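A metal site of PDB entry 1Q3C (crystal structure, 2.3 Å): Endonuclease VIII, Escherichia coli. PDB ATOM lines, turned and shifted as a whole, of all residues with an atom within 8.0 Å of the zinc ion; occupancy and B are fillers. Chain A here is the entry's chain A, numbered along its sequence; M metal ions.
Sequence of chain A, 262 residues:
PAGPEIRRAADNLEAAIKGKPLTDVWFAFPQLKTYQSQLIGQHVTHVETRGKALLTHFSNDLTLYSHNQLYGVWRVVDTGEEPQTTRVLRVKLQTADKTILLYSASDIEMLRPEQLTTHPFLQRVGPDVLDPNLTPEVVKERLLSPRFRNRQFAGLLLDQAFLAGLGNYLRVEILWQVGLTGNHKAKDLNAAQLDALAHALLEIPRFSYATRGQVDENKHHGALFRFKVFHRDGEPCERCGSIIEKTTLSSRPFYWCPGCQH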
ATOM      1  N   TRP A 176      -5.077 -28.772  -2.239  1.00  0.00           N
ATOM      2  CA  TRP A 176      -6.157 -27.805  -2.066  1.00  0.00           C
ATOM      3  C   TRP A 176      -6.283 -26.928  -3.298  1.00  0.00           C
ATOM      4  O   TRP A 176      -7.380 -26.523  -3.652  1.00  0.00           O
ATOM      5  CB  TRP A 176      -5.891 -26.899  -0.868  1.00  0.00           C
ATOM      6  CG  TRP A 176      -7.015 -25.946  -0.612  1.00  0.00           C
ATOM      7  CD1 TRP A 176      -8.195 -26.212   0.033  1.00  0.00           C
ATOM      8  CD2 TRP A 176      -7.073 -24.561  -1.015  1.00  0.00           C
ATOM      9  NE1 TRP A 176      -8.980 -25.083   0.061  1.00  0.00           N
ATOM     10  CE2 TRP A 176      -8.321 -24.056  -0.561  1.00  0.00           C
ATOM     11  CE3 TRP A 176      -6.210 -23.712  -1.696  1.00  0.00           C
ATOM     12  CZ2 TRP A 176      -8.714 -22.732  -0.782  1.00  0.00           C
ATOM     13  CZ3 TRP A 176      -6.601 -22.391  -1.908  1.00  0.00           C
ATOM     14  CH2 TRP A 176      -7.836 -21.912  -1.450  1.00  0.00           C
ATOM     15  N   VAL A 229      -4.393 -24.414   4.071  1.00  0.00           N
ATOM     16  CA  VAL A 229      -4.935 -25.476   4.901  1.00  0.00           C
ATOM     17  C   VAL A 229      -3.887 -26.106   5.826  1.00  0.00           C
ATOM     18  O   VAL A 229      -4.232 -26.896   6.698  1.00  0.00           O
ATOM     19  CB  VAL A 229      -5.571 -26.580   4.042  1.00  0.00           C
ATOM     20  CG1 VAL A 229      -6.684 -25.999   3.195  1.00  0.00           C
ATOM     21  CG2 VAL A 229      -4.505 -27.245   3.167  1.00  0.00           C
ATOM     22  N   PRO A 236     -12.031 -21.337   8.687  1.00  0.00           N
ATOM     23  CA  PRO A 236     -12.768 -21.405   7.422  1.00  0.00           C
ATOM     24  C   PRO A 236     -11.856 -21.414   6.215  1.00  0.00           C
ATOM     25  O   PRO A 236     -10.716 -20.968   6.282  1.00  0.00           O
ATOM     26  CB  PRO A 236     -13.653 -20.155   7.476  1.00  0.00           C
ATOM     27  CG  PRO A 236     -12.800 -19.192   8.232  1.00  0.00           C
ATOM     28  CD  PRO A 236     -12.243 -20.040   9.348  1.00  0.00           C
ATOM     29  N   CYS A 237     -12.371 -21.944   5.114  1.00  0.00           N
ATOM     30  CA  CYS A 237     -11.653 -22.023   3.857  1.00  0.00           C
ATOM     31  C   CYS A 237     -11.871 -20.695   3.126  1.00  0.00           C
ATOM     32  O   CYS A 237     -12.960 -20.134   3.157  1.00  0.00           O
ATOM     33  CB  CYS A 237     -12.209 -23.202   3.035  1.00  0.00           C
ATOM     34  SG  CYS A 237     -11.839 -23.162   1.281  1.00  0.00           S
ATOM     35  N   GLU A 238     -10.819 -20.180   2.497  1.00  0.00           N
ATOM     36  CA  GLU A 238     -10.922 -18.904   1.795  1.00  0.00           C
ATOM     37  C   GLU A 238     -11.845 -18.989   0.585  1.00  0.00           C
ATOM     38  O   GLU A 238     -12.394 -17.987   0.130  1.00  0.00           O
ATOM     39  CB  GLU A 238      -9.546 -18.417   1.346  1.00  0.00           C
ATOM     40  CG  GLU A 238      -9.039 -19.005   0.035  1.00  0.00           C
ATOM     41  CD  GLU A 238      -7.793 -18.306  -0.478  1.00  0.00           C
ATOM     42  OE1 GLU A 238      -7.107 -17.631   0.321  1.00  0.00           O
ATOM     43  OE2 GLU A 238      -7.498 -18.425  -1.685  1.00  0.00           O
ATOM     44  N   ARG A 239     -11.998 -20.201   0.058  1.00  0.00           N
ATOM     45  CA  ARG A 239     -12.834 -20.449  -1.114  1.00  0.00           C
ATOM     46  C   ARG A 239     -14.329 -20.605  -0.806  1.00  0.00           C
ATOM     47  O   ARG A 239     -15.131 -19.721  -1.130  1.00  0.00           O
ATOM     48  CB  ARG A 239     -12.304 -21.705  -1.826  1.00  0.00           C
ATOM     49  CG  ARG A 239     -13.018 -22.141  -3.094  1.00  0.00           C
ATOM     50  CD  ARG A 239     -12.315 -23.404  -3.556  1.00  0.00           C
ATOM     51  NE  ARG A 239     -12.846 -24.047  -4.763  1.00  0.00           N
ATOM     52  CZ  ARG A 239     -12.941 -23.464  -5.951  1.00  0.00           C
ATOM     53  NH1 ARG A 239     -12.574 -22.194  -6.111  1.00  0.00           N
ATOM     54  NH2 ARG A 239     -13.342 -24.178  -7.001  1.00  0.00           N
ATOM     55  N   CYS A 240     -14.701 -21.703  -0.165  1.00  0.00           N
ATOM     56  CA  CYS A 240     -16.092 -21.976   0.138  1.00  0.00           C
ATOM     57  C   CYS A 240     -16.568 -21.596   1.544  1.00  0.00           C
ATOM     58  O   CYS A 240     -17.761 -21.446   1.770  1.00  0.00           O
ATOM     59  CB  CYS A 240     -16.375 -23.454  -0.076  1.00  0.00           C
ATOM     60  SG  CYS A 240     -15.490 -24.478   1.105  1.00  0.00           S
ATOM     61  N   GLY A 241     -15.641 -21.459   2.488  1.00  0.00           N
ATOM     62  CA  GLY A 241     -16.023 -21.085   3.831  1.00  0.00           C
ATOM     63  C   GLY A 241     -16.161 -22.246   4.808  1.00  0.00           C
ATOM     64  O   GLY A 241     -16.411 -22.032   6.000  1.00  0.00           O
ATOM     65  N   SER A 242     -15.996 -23.468   4.322  1.00  0.00           N
ATOM     66  CA  SER A 242     -16.114 -24.643   5.180  1.00  0.00           C
ATOM     67  C   SER A 242     -14.934 -24.703   6.138  1.00  0.00           C
ATOM     68  O   SER A 242     -13.862 -24.158   5.864  1.00  0.00           O
ATOM     69  CB  SER A 242     -16.153 -25.913   4.342  1.00  0.00           C
ATOM     70  OG  SER A 242     -17.220 -25.884   3.417  1.00  0.00           O
ATOM     71  N   ILE A 243     -15.125 -25.379   7.270  1.00  0.00           N
ATOM     72  CA  ILE A 243     -14.070 -25.492   8.259  1.00  0.00           C
ATOM     73  C   ILE A 243     -13.025 -26.529   7.847  1.00  0.00           C
ATOM     74  O   ILE A 243     -13.366 -27.674   7.548  1.00  0.00           O
ATOM     75  CB  ILE A 243     -14.656 -25.841   9.644  1.00  0.00           C
ATOM     76  CG1 ILE A 243     -15.699 -24.792  10.048  1.00  0.00           C
ATOM     77  CG2 ILE A 243     -13.544 -25.928  10.685  1.00  0.00           C
ATOM     78  CD1 ILE A 243     -15.212 -23.345   9.938  1.00  0.00           C
ATOM     79  N   ILE A 244     -11.759 -26.115   7.834  1.00  0.00           N
ATOM     80  CA  ILE A 244     -10.667 -27.004   7.461  1.00  0.00           C
ATOM     81  C   ILE A 244     -10.444 -28.078   8.516  1.00  0.00           C
ATOM     82  O   ILE A 244     -10.512 -27.814   9.714  1.00  0.00           O
ATOM     83  CB  ILE A 244      -9.365 -26.203   7.265  1.00  0.00           C
ATOM     84  CG1 ILE A 244      -9.605 -25.071   6.265  1.00  0.00           C
ATOM     85  CG2 ILE A 244      -8.249 -27.128   6.769  1.00  0.00           C
ATOM     86  CD1 ILE A 244      -8.405 -24.172   6.049  1.00  0.00           C
ATOM     87  N   TRP A 256      -7.222 -30.400   4.929  1.00  0.00           N
ATOM     88  CA  TRP A 256      -8.047 -30.151   3.754  1.00  0.00           C
ATOM     89  C   TRP A 256      -9.394 -29.544   4.066  1.00  0.00           C
ATOM     90  O   TRP A 256      -9.857 -29.543   5.210  1.00  0.00           O
ATOM     91  CB  TRP A 256      -8.271 -31.455   2.998  1.00  0.00           C
ATOM     92  CG  TRP A 256      -9.359 -32.300   3.576  1.00  0.00           C
ATOM     93  CD1 TRP A 256     -10.623 -32.464   3.079  1.00  0.00           C
ATOM     94  CD2 TRP A 256      -9.303 -33.048   4.802  1.00  0.00           C
ATOM     95  NE1 TRP A 256     -11.348 -33.281   3.919  1.00  0.00           N
ATOM     96  CE2 TRP A 256     -10.565 -33.654   4.978  1.00  0.00           C
ATOM     97  CE3 TRP A 256      -8.303 -33.267   5.762  1.00  0.00           C
ATOM     98  CZ2 TRP A 256     -10.859 -34.462   6.078  1.00  0.00           C
ATOM     99  CZ3 TRP A 256      -8.598 -34.072   6.854  1.00  0.00           C
ATOM    100  CH2 TRP A 256      -9.869 -34.660   7.003  1.00  0.00           C
ATOM    101  N   CYS A 257     -10.018 -29.021   3.027  1.00  0.00           N
ATOM    102  CA  CYS A 257     -11.358 -28.462   3.132  1.00  0.00           C
ATOM    103  C   CYS A 257     -12.292 -29.541   2.604  1.00  0.00           C
ATOM    104  O   CYS A 257     -12.269 -29.855   1.410  1.00  0.00           O
ATOM    105  CB  CYS A 257     -11.496 -27.201   2.296  1.00  0.00           C
ATOM    106  SG  CYS A 257     -13.218 -26.640   2.231  1.00  0.00           S
ATOM    107  N   PRO A 258     -13.110 -30.144   3.480  1.00  0.00           N
ATOM    108  CA  PRO A 258     -14.039 -31.179   3.045  1.00  0.00           C
ATOM    109  C   PRO A 258     -15.169 -30.538   2.253  1.00  0.00           C
ATOM    110  O   PRO A 258     -16.048 -31.216   1.708  1.00  0.00           O
ATOM    111  CB  PRO A 258     -14.507 -31.784   4.361  1.00  0.00           C
ATOM    112  CG  PRO A 258     -14.551 -30.586   5.263  1.00  0.00           C
ATOM    113  CD  PRO A 258     -13.260 -29.861   4.926  1.00  0.00           C
ATOM    114  N   GLY A 259     -15.127 -29.208   2.189  1.00  0.00           N
ATOM    115  CA  GLY A 259     -16.131 -28.450   1.464  1.00  0.00           C
ATOM    116  C   GLY A 259     -15.886 -28.401  -0.030  1.00  0.00           C
ATOM    117  O   GLY A 259     -16.779 -28.729  -0.814  1.00  0.00           O
ATOM    118  N   CYS A 260     -14.682 -27.985  -0.448  1.00  0.00           N
ATOM    119  CA  CYS A 260     -14.389 -27.910  -1.879  1.00  0.00           C
ATOM    120  C   CYS A 260     -13.297 -28.879  -2.382  1.00  0.00           C
ATOM    121  O   CYS A 260     -12.769 -28.707  -3.483  1.00  0.00           O
ATOM    122  CB  CYS A 260     -14.052 -26.466  -2.274  1.00  0.00           C
ATOM    123  SG  CYS A 260     -12.695 -25.742  -1.361  1.00  0.00           S
ATOM    124  N   GLN A 261     -12.958 -29.885  -1.580  1.00  0.00           N
ATOM    125  CA  GLN A 261     -11.959 -30.867  -1.985  1.00  0.00           C
ATOM    126  C   GLN A 261     -12.579 -32.255  -2.025  1.00  0.00           C
ATOM    127  O   GLN A 261     -13.160 -32.707  -1.044  1.00  0.00           O
ATOM    128  CB  GLN A 261     -10.770 -30.856  -1.022  1.00  0.00           C
ATOM    129  CG  GLN A 261      -9.630 -29.937  -1.465  1.00  0.00           C
ATOM    130  CD  GLN A 261      -8.450 -29.924  -0.501  1.00  0.00           C
ATOM    131  OE1 GLN A 261      -8.482 -29.244   0.530  1.00  0.00           O
ATOM    132  NE2 GLN A 261      -7.410 -30.690  -0.820  1.00  0.00           N
HETATM  133 ZN    ZN M   1     -13.199 -25.066   0.690  1.00  0.00          ZN
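The side-chain sulfur (SG) of Cys 257 lies close to the backbone NH (N) of Gly 259, at 3.2 Å. The side-chain amide oxygen (OE1) of Gln 261 sits at hydrogen-bond distance from the backbone NH (N) of Cys 257, at 2.9 Å. The side-chain sulfur (SG) of Cys 240 sits close to the side-chain hydroxyl (OG) of Ser 242, 3.2 Å away. The side-chain sulfur (SG) of Cys 237 lies close to the indole nitrogen (NE1) of Trp 176 (3.7 Å). The side-chain sulfur (SG) of Cys 237 lies close to the backbone NH (N) of Arg 239, at 3.2 Å. The backbone carbonyl oxygen (O) of Ser 242 lies within hydrogen-bond range of the backbone NH (N) of Cys 237, at 2.8 Å.
Within 4 Å of the zinc ion: Cys 237, Cys 240, Cys 257 and Cys 260.
The zinc ion is bound by SG of Cys 257 (2.2 Å), SG of Cys 260 (2.2 Å), SG of Cys 240 (2.4 Å) and SG of Cys 237 (2.4 Å).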
